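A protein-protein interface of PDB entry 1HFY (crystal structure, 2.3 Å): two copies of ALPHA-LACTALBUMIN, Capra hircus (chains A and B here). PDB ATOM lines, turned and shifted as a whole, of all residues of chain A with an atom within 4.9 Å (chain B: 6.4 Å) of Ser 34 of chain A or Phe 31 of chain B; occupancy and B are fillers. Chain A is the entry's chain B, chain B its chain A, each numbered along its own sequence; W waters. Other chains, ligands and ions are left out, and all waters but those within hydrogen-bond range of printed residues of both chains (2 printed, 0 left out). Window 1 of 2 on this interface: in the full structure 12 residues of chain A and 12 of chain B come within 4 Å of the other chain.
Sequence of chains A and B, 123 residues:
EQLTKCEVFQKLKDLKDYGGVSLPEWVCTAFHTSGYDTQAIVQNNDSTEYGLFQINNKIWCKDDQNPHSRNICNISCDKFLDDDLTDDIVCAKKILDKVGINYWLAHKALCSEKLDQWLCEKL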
ATOM      1  N   ALA A  30     -19.350  -8.293 -27.220  1.00  0.00           N
ATOM      2  CA  ALA A  30     -18.378  -8.956 -28.091  1.00  0.00           C
ATOM      3  C   ALA A  30     -17.800 -10.192 -27.424  1.00  0.00           C
ATOM      4  O   ALA A  30     -17.526 -11.188 -28.107  1.00  0.00           O
ATOM      5  CB  ALA A  30     -17.256  -8.002 -28.458  1.00  0.00           C
ATOM      6  N   PHE A  31     -17.559 -10.104 -26.115  1.00  0.00           N
ATOM      7  CA  PHE A  31     -17.025 -11.217 -25.333  1.00  0.00           C
ATOM      8  C   PHE A  31     -17.977 -12.373 -25.435  1.00  0.00           C
ATOM      9  O   PHE A  31     -17.605 -13.470 -25.838  1.00  0.00           O
ATOM     10  CB  PHE A  31     -16.909 -10.850 -23.857  1.00  0.00           C
ATOM     11  CG  PHE A  31     -16.513 -12.008 -22.970  1.00  0.00           C
ATOM     12  CD1 PHE A  31     -15.258 -12.604 -23.090  1.00  0.00           C
ATOM     13  CD2 PHE A  31     -17.418 -12.535 -22.046  1.00  0.00           C
ATOM     14  CE1 PHE A  31     -14.922 -13.716 -22.302  1.00  0.00           C
ATOM     15  CE2 PHE A  31     -17.089 -13.655 -21.251  1.00  0.00           C
ATOM     16  CZ  PHE A  31     -15.852 -14.238 -21.383  1.00  0.00           C
ATOM     17  N   HIS A  32     -19.228 -12.107 -25.106  1.00  0.00           N
ATOM     18  CA  HIS A  32     -20.252 -13.134 -25.124  1.00  0.00           C
ATOM     19  C   HIS A  32     -20.659 -13.685 -26.492  1.00  0.00           C
ATOM     20  O   HIS A  32     -21.189 -14.789 -26.562  1.00  0.00           O
ATOM     21  CB  HIS A  32     -21.487 -12.640 -24.373  1.00  0.00           C
ATOM     22  CG  HIS A  32     -21.284 -12.532 -22.895  1.00  0.00           C
ATOM     23  ND1 HIS A  32     -21.215 -13.637 -22.073  1.00  0.00           N
ATOM     24  CD2 HIS A  32     -21.124 -11.454 -22.088  1.00  0.00           C
ATOM     25  CE1 HIS A  32     -21.023 -13.242 -20.828  1.00  0.00           C
ATOM     26  NE2 HIS A  32     -20.966 -11.925 -20.808  1.00  0.00           N
ATOM     27  N   THR A  33     -20.382 -12.939 -27.560  1.00  0.00           N
ATOM     28  CA  THR A  33     -20.739 -13.301 -28.933  1.00  0.00           C
ATOM     29  C   THR A  33     -19.644 -14.063 -29.665  1.00  0.00           C
ATOM     30  O   THR A  33     -19.895 -15.118 -30.241  1.00  0.00           O
ATOM     31  CB  THR A  33     -21.101 -12.010 -29.744  1.00  0.00           C
ATOM     32  OG1 THR A  33     -22.277 -11.417 -29.183  1.00  0.00           O
ATOM     33  CG2 THR A  33     -21.337 -12.299 -31.193  1.00  0.00           C
ATOM     34  N   SER A  34     -18.429 -13.540 -29.652  1.00  0.00           N
ATOM     35  CA  SER A  34     -17.359 -14.213 -30.354  1.00  0.00           C
ATOM     36  C   SER A  34     -16.098 -14.462 -29.526  1.00  0.00           C
ATOM     37  O   SER A  34     -15.144 -15.043 -30.028  1.00  0.00           O
ATOM     38  CB  SER A  34     -16.996 -13.386 -31.563  1.00  0.00           C
ATOM     39  OG  SER A  34     -16.623 -12.095 -31.135  1.00  0.00           O
ATOM     40  N   GLY A  35     -16.094 -14.044 -28.264  1.00  0.00           N
ATOM     41  CA  GLY A  35     -14.907 -14.205 -27.444  1.00  0.00           C
ATOM     42  C   GLY A  35     -13.774 -13.316 -27.951  1.00  0.00           C
ATOM     43  O   GLY A  35     -12.618 -13.608 -27.692  1.00  0.00           O
ATOM     44  N   TYR A  36     -14.111 -12.210 -28.632  1.00  0.00           N
ATOM     45  CA  TYR A  36     -13.123 -11.281 -29.208  1.00  0.00           C
ATOM     46  C   TYR A  36     -12.365 -11.829 -30.432  1.00  0.00           C
ATOM     47  O   TYR A  36     -11.269 -11.362 -30.733  1.00  0.00           O
ATOM     48  CB  TYR A  36     -12.063 -10.851 -28.187  1.00  0.00           C
ATOM     49  CG  TYR A  36     -12.571 -10.276 -26.907  1.00  0.00           C
ATOM     50  CD1 TYR A  36     -13.704  -9.470 -26.865  1.00  0.00           C
ATOM     51  CD2 TYR A  36     -11.906 -10.536 -25.720  1.00  0.00           C
ATOM     52  CE1 TYR A  36     -14.167  -8.935 -25.654  1.00  0.00           C
ATOM     53  CE2 TYR A  36     -12.355 -10.006 -24.515  1.00  0.00           C
ATOM     54  CZ  TYR A  36     -13.487  -9.213 -24.488  1.00  0.00           C
ATOM     55  OH  TYR A  36     -13.940  -8.756 -23.265  1.00  0.00           O
ATOM     56  N   ASP A  37     -12.913 -12.801 -31.147  1.00  0.00           N
ATOM     57  CA  ASP A  37     -12.205 -13.344 -32.311  1.00  0.00           C
ATOM     58  C   ASP A  37     -12.812 -12.796 -33.594  1.00  0.00           C
ATOM     59  O   ASP A  37     -13.959 -13.080 -33.878  1.00  0.00           O
ATOM     60  CB  ASP A  37     -12.329 -14.858 -32.295  1.00  0.00           C
ATOM     61  CG  ASP A  37     -11.602 -15.532 -33.435  1.00  0.00           C
ATOM     62  OD1 ASP A  37     -10.919 -14.859 -34.248  1.00  0.00           O
ATOM     63  OD2 ASP A  37     -11.719 -16.773 -33.513  1.00  0.00           O
ATOM     64  N   ALA A  40     -14.173 -15.675 -36.148  1.00  0.00           N
ATOM     65  CA  ALA A  40     -15.137 -16.690 -35.732  1.00  0.00           C
ATOM     66  C   ALA A  40     -16.198 -16.812 -36.795  1.00  0.00           C
ATOM     67  O   ALA A  40     -16.569 -15.818 -37.411  1.00  0.00           O
ATOM     68  CB  ALA A  40     -15.785 -16.310 -34.396  1.00  0.00           C
ATOM     69  N   VAL A  42     -19.648 -19.436 -37.112  1.00  0.00           N
ATOM     70  CA  VAL A  42     -20.394 -20.482 -36.436  1.00  0.00           C
ATOM     71  C   VAL A  42     -21.559 -20.921 -37.319  1.00  0.00           C
ATOM     72  O   VAL A  42     -22.311 -20.093 -37.814  1.00  0.00           O
ATOM     73  CB  VAL A  42     -20.898 -20.006 -35.049  1.00  0.00           C
ATOM     74  CG1 VAL A  42     -21.917 -20.988 -34.483  1.00  0.00           C
ATOM     75  CG2 VAL A  42     -19.735 -19.852 -34.104  1.00  0.00           C
ATOM     76  N   GLY A  51     -17.600 -13.375 -37.980  1.00  0.00           N
ATOM     77  CA  GLY A  51     -16.842 -12.430 -37.193  1.00  0.00           C
ATOM     78  C   GLY A  51     -17.254 -12.073 -35.784  1.00  0.00           C
ATOM     79  O   GLY A  51     -18.080 -12.740 -35.171  1.00  0.00           O
ATOM     80  N   LEU A  52     -16.670 -10.969 -35.310  1.00  0.00           N
ATOM     81  CA  LEU A  52     -16.857 -10.397 -33.982  1.00  0.00           C
ATOM     82  C   LEU A  52     -18.309 -10.250 -33.568  1.00  0.00           C
ATOM     83  O   LEU A  52     -18.660 -10.541 -32.423  1.00  0.00           O
ATOM     84  CB  LEU A  52     -16.158  -9.019 -33.915  1.00  0.00           C
ATOM     85  CG  LEU A  52     -15.770  -8.407 -32.545  1.00  0.00           C
ATOM     86  CD1 LEU A  52     -14.540  -9.125 -31.979  1.00  0.00           C
ATOM     87  CD2 LEU A  52     -15.452  -6.918 -32.650  1.00  0.00           C
ATOM     88  N   PHE A  53     -19.143  -9.767 -34.493  1.00  0.00           N
ATOM     89  CA  PHE A  53     -20.572  -9.546 -34.216  1.00  0.00           C
ATOM     90  C   PHE A  53     -21.457 -10.678 -34.674  1.00  0.00           C
ATOM     91  O   PHE A  53     -22.673 -10.546 -34.660  1.00  0.00           O
ATOM     92  CB  PHE A  53     -21.056  -8.240 -34.861  1.00  0.00           C
ATOM     93  CG  PHE A  53     -20.424  -7.002 -34.257  1.00  0.00           C
ATOM     94  CD1 PHE A  53     -20.646  -6.672 -32.912  1.00  0.00           C
ATOM     95  CD2 PHE A  53     -19.550  -6.222 -34.992  1.00  0.00           C
ATOM     96  CE1 PHE A  53     -19.993  -5.590 -32.320  1.00  0.00           C
ATOM     97  CE2 PHE A  53     -18.899  -5.144 -34.409  1.00  0.00           C
ATOM     98  CZ  PHE A  53     -19.115  -4.827 -33.081  1.00  0.00           C
ATOM     99  N   GLN A  54     -20.847 -11.791 -35.070  1.00  0.00           N
ATOM    100  CA  GLN A  54     -21.584 -12.958 -35.553  1.00  0.00           C
ATOM    101  C   GLN A  54     -22.785 -12.551 -36.392  1.00  0.00           C
ATOM    102  O   GLN A  54     -23.952 -12.831 -36.052  1.00  0.00           O
ATOM    103  CB  GLN A  54     -21.975 -13.889 -34.392  1.00  0.00           C
ATOM    104  CG  GLN A  54     -20.775 -14.618 -33.752  1.00  0.00           C
ATOM    105  CD  GLN A  54     -20.158 -15.692 -34.646  1.00  0.00           C
ATOM    106  OE1 GLN A  54     -20.744 -16.742 -34.844  1.00  0.00           O
ATOM    107  NE2 GLN A  54     -18.973 -15.421 -35.195  1.00  0.00           N
ATOM    108  N   TRP B  26     -17.898 -30.352 -26.241  1.00  0.00           N
ATOM    109  CA  TRP B  26     -17.149 -29.721 -25.153  1.00  0.00           C
ATOM    110  C   TRP B  26     -16.436 -28.451 -25.635  1.00  0.00           C
ATOM    111  O   TRP B  26     -16.489 -27.414 -24.969  1.00  0.00           O
ATOM    112  CB  TRP B  26     -16.129 -30.701 -24.540  1.00  0.00           C
ATOM    113  CG  TRP B  26     -16.743 -31.617 -23.516  1.00  0.00           C
ATOM    114  CD1 TRP B  26     -16.921 -32.971 -23.624  1.00  0.00           C
ATOM    115  CD2 TRP B  26     -17.371 -31.226 -22.279  1.00  0.00           C
ATOM    116  NE1 TRP B  26     -17.652 -33.450 -22.544  1.00  0.00           N
ATOM    117  CE2 TRP B  26     -17.940 -32.405 -21.703  1.00  0.00           C
ATOM    118  CE3 TRP B  26     -17.529 -29.999 -21.606  1.00  0.00           C
ATOM    119  CZ2 TRP B  26     -18.642 -32.388 -20.488  1.00  0.00           C
ATOM    120  CZ3 TRP B  26     -18.228 -29.978 -20.406  1.00  0.00           C
ATOM    121  CH2 TRP B  26     -18.782 -31.169 -19.855  1.00  0.00           C
ATOM    122  N   VAL B  27     -15.803 -28.511 -26.804  1.00  0.00           N
ATOM    123  CA  VAL B  27     -15.090 -27.355 -27.383  1.00  0.00           C
ATOM    124  C   VAL B  27     -16.054 -26.238 -27.742  1.00  0.00           C
ATOM    125  O   VAL B  27     -15.723 -25.060 -27.621  1.00  0.00           O
ATOM    126  CB  VAL B  27     -14.259 -27.753 -28.623  1.00  0.00           C
ATOM    127  CG1 VAL B  27     -15.134 -28.491 -29.589  1.00  0.00           C
ATOM    128  CG2 VAL B  27     -13.642 -26.523 -29.317  1.00  0.00           C
ATOM    129  N   CYS B  28     -17.262 -26.611 -28.134  1.00  0.00           N
ATOM    130  CA  CYS B  28     -18.317 -25.667 -28.483  1.00  0.00           C
ATOM    131  C   CYS B  28     -18.805 -24.905 -27.232  1.00  0.00           C
ATOM    132  O   CYS B  28     -18.979 -23.675 -27.256  1.00  0.00           O
ATOM    133  CB  CYS B  28     -19.455 -26.455 -29.127  1.00  0.00           C
ATOM    134  SG  CYS B  28     -20.935 -25.517 -29.565  1.00  0.00           S
ATOM    135  N   THR B  29     -18.967 -25.656 -26.136  1.00  0.00           N
ATOM    136  CA  THR B  29     -19.396 -25.137 -24.847  1.00  0.00           C
ATOM    137  C   THR B  29     -18.338 -24.177 -24.356  1.00  0.00           C
ATOM    138  O   THR B  29     -18.639 -23.155 -23.783  1.00  0.00           O
ATOM    139  CB  THR B  29     -19.548 -26.289 -23.809  1.00  0.00           C
ATOM    140  OG1 THR B  29     -20.583 -27.184 -24.223  1.00  0.00           O
ATOM    141  CG2 THR B  29     -19.905 -25.742 -22.449  1.00  0.00           C
ATOM    142  N   ALA B  30     -17.083 -24.513 -24.592  1.00  0.00           N
ATOM    143  CA  ALA B  30     -15.990 -23.661 -24.171  1.00  0.00           C
ATOM    144  C   ALA B  30     -15.963 -22.360 -24.960  1.00  0.00           C
ATOM    145  O   ALA B  30     -15.603 -21.336 -24.414  1.00  0.00           O
ATOM    146  CB  ALA B  30     -14.650 -24.396 -24.295  1.00  0.00           C
ATOM    147  N   PHE B  31     -16.275 -22.416 -26.252  1.00  0.00           N
ATOM    148  CA  PHE B  31     -16.291 -21.221 -27.099  1.00  0.00           C
ATOM    149  C   PHE B  31     -17.350 -20.251 -26.630  1.00  0.00           C
ATOM    150  O   PHE B  31     -17.102 -19.066 -26.487  1.00  0.00           O
ATOM    151  CB  PHE B  31     -16.619 -21.570 -28.552  1.00  0.00           C
ATOM    152  CG  PHE B  31     -16.772 -20.364 -29.453  1.00  0.00           C
ATOM    153  CD1 PHE B  31     -15.659 -19.642 -29.869  1.00  0.00           C
ATOM    154  CD2 PHE B  31     -18.031 -19.941 -29.873  1.00  0.00           C
ATOM    155  CE1 PHE B  31     -15.801 -18.518 -30.688  1.00  0.00           C
ATOM    156  CE2 PHE B  31     -18.192 -18.811 -30.697  1.00  0.00           C
ATOM    157  CZ  PHE B  31     -17.072 -18.105 -31.099  1.00  0.00           C
ATOM    158  N   HIS B  32     -18.550 -20.761 -26.432  1.00  0.00           N
ATOM    159  CA  HIS B  32     -19.648 -19.935 -26.007  1.00  0.00           C
ATOM    160  C   HIS B  32     -19.563 -19.455 -24.575  1.00  0.00           C
ATOM    161  O   HIS B  32     -20.244 -18.504 -24.190  1.00  0.00           O
ATOM    162  CB  HIS B  32     -20.936 -20.703 -26.176  1.00  0.00           C
ATOM    163  CG  HIS B  32     -21.322 -20.904 -27.594  1.00  0.00           C
ATOM    164  ND1 HIS B  32     -21.821 -19.889 -28.374  1.00  0.00           N
ATOM    165  CD2 HIS B  32     -21.301 -22.010 -28.376  1.00  0.00           C
ATOM    166  CE1 HIS B  32     -22.099 -20.359 -29.574  1.00  0.00           C
ATOM    167  NE2 HIS B  32     -21.791 -21.644 -29.600  1.00  0.00           N
ATOM    168  N   THR B  33     -18.745 -20.122 -23.779  1.00  0.00           N
ATOM    169  CA  THR B  33     -18.619 -19.775 -22.381  1.00  0.00           C
ATOM    170  C   THR B  33     -17.586 -18.712 -22.046  1.00  0.00           C
ATOM    171  O   THR B  33     -17.910 -17.768 -21.364  1.00  0.00           O
ATOM    172  CB  THR B  33     -18.369 -21.060 -21.554  1.00  0.00           C
ATOM    173  OG1 THR B  33     -19.525 -21.889 -21.637  1.00  0.00           O
ATOM    174  CG2 THR B  33     -18.109 -20.754 -20.118  1.00  0.00           C
ATOM    175  N   SER B  34     -16.356 -18.856 -22.533  1.00  0.00           N
ATOM    176  CA  SER B  34     -15.271 -17.928 -22.210  1.00  0.00           C
ATOM    177  C   SER B  34     -14.427 -17.601 -23.404  1.00  0.00           C
ATOM    178  O   SER B  34     -13.397 -16.949 -23.263  1.00  0.00           O
ATOM    179  CB  SER B  34     -14.354 -18.583 -21.185  1.00  0.00           C
ATOM    180  OG  SER B  34     -13.835 -19.779 -21.751  1.00  0.00           O
ATOM    181  N   GLY B  35     -14.828 -18.116 -24.566  1.00  0.00           N
ATOM    182  CA  GLY B  35     -14.086 -17.889 -25.802  1.00  0.00           C
ATOM    183  C   GLY B  35     -12.688 -18.506 -25.827  1.00  0.00           C
ATOM    184  O   GLY B  35     -11.843 -18.018 -26.575  1.00  0.00           O
ATOM    185  N   TYR B  36     -12.483 -19.595 -25.070  1.00  0.00           N
ATOM    186  CA  TYR B  36     -11.205 -20.319 -24.948  1.00  0.00           C
ATOM    187  C   TYR B  36     -10.189 -19.564 -24.088  1.00  0.00           C
ATOM    188  O   TYR B  36      -8.991 -19.776 -24.213  1.00  0.00           O
ATOM    189  CB  TYR B  36     -10.567 -20.604 -26.317  1.00  0.00           C
ATOM    190  CG  TYR B  36     -11.457 -21.297 -27.357  1.00  0.00           C
ATOM    191  CD1 TYR B  36     -12.337 -22.311 -27.000  1.00  0.00           C
ATOM    192  CD2 TYR B  36     -11.386 -20.938 -28.711  1.00  0.00           C
ATOM    193  CE1 TYR B  36     -13.125 -22.959 -27.948  1.00  0.00           C
ATOM    194  CE2 TYR B  36     -12.170 -21.583 -29.671  1.00  0.00           C
ATOM    195  CZ  TYR B  36     -13.041 -22.601 -29.284  1.00  0.00           C
ATOM    196  OH  TYR B  36     -13.822 -23.264 -30.244  1.00  0.00           O
ATOM    197  N   TRP B 118     -16.481 -28.200 -34.915  1.00  0.00           N
ATOM    198  CA  TRP B 118     -15.694 -28.099 -33.696  1.00  0.00           C
ATOM    199  C   TRP B 118     -14.525 -29.085 -33.675  1.00  0.00           C
ATOM    200  O   TRP B 118     -13.737 -29.115 -32.728  1.00  0.00           O
ATOM    201  CB  TRP B 118     -16.619 -28.341 -32.507  1.00  0.00           C
ATOM    202  CG  TRP B 118     -17.707 -27.367 -32.477  1.00  0.00           C
ATOM    203  CD1 TRP B 118     -19.017 -27.608 -32.671  1.00  0.00           C
ATOM    204  CD2 TRP B 118     -17.576 -25.950 -32.270  1.00  0.00           C
ATOM    205  NE1 TRP B 118     -19.725 -26.433 -32.602  1.00  0.00           N
ATOM    206  CE2 TRP B 118     -18.862 -25.398 -32.358  1.00  0.00           C
ATOM    207  CE3 TRP B 118     -16.488 -25.098 -32.013  1.00  0.00           C
ATOM    208  CZ2 TRP B 118     -19.105 -24.020 -32.202  1.00  0.00           C
ATOM    209  CZ3 TRP B 118     -16.727 -23.728 -31.855  1.00  0.00           C
ATOM    210  CH2 TRP B 118     -18.024 -23.205 -31.952  1.00  0.00           C
HETATM  211  O   HOH W   1     -21.241 -17.082 -27.486  1.00  0.00           O
HETATM  212  O   HOH W   2     -23.073 -16.974 -24.685  1.00  0.00           O
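Printed residues of chain B that touch a printed residue of chain A: Phe 31 and Ser 34. Among the printed residues, no Asp or Glu carboxylate lies within 4 Å of a Lys or Arg side-chain nitrogen of the other chain.
Phe 31 of chain A touches Ser 34 of chain B, and with the chains exchanged Ser 34 of chain A touches Phe 31 of chain B. 7 positions are printed for both chains.
Water W1 bridges the backbone carbonyl oxygen of His 32 of chain A and a ring nitrogen (ND1) of His 32 of chain B. Water W2 bridges the backbone carbonyl oxygen of His 32 of chain B (3.3 Å) and the backbone carbonyl oxygen of His 32 of chain A (3.4 Å).
Printed residues of chain B within 4 Å of Phe 31 of chain A: Ser 34. Of chain B, only Phe 31 comes within 4 Å of Ser 34 of chain A. Of the printed residues of chain B, Ala 40 of chain A touches Phe 31. Of chain A, only Ser 34, Ala 40 and Val 42 come within 4 Å of Phe 31 of chain B. The nearest residue of chain B that does not touch Ser 34 of chain A is Gly 35 of chain B (5.2 Å).
The backbone carbonyl oxygen (O) of Ala 30 of chain A sits at hydrogen-bond distance from the side-chain hydroxyl (OG) of Ser 34 of chain A. The side-chain hydroxyl (OG) of Ser 34 of chain A lies within hydrogen-bond range of the backbone carbonyl oxygen (O) of Leu 52 of chain A, 2.9 Å away. O of Ala 40 of chain A is in hydrogen-bond range of N of Gly 51 of chain A, 2.7 Å away. The side-chain amide nitrogen (NE2) of Gln 54 of chain A is in hydrogen-bond range of the backbone carbonyl oxygen (O) of Ala 40 of chain A (3.3 Å).
Among the printed residues, pairs that only touch across the chains: Ser 34 of chain A with Phe 31 of chain B (3.6 Å), Phe 31 of chain A with Ser 34 of chain B (3.7 Å), Val 42 of chain A with Phe 31 of chain B (3.9 Å) and Ala 40 of chain A with Phe 31 of chain B (3.97 Å).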
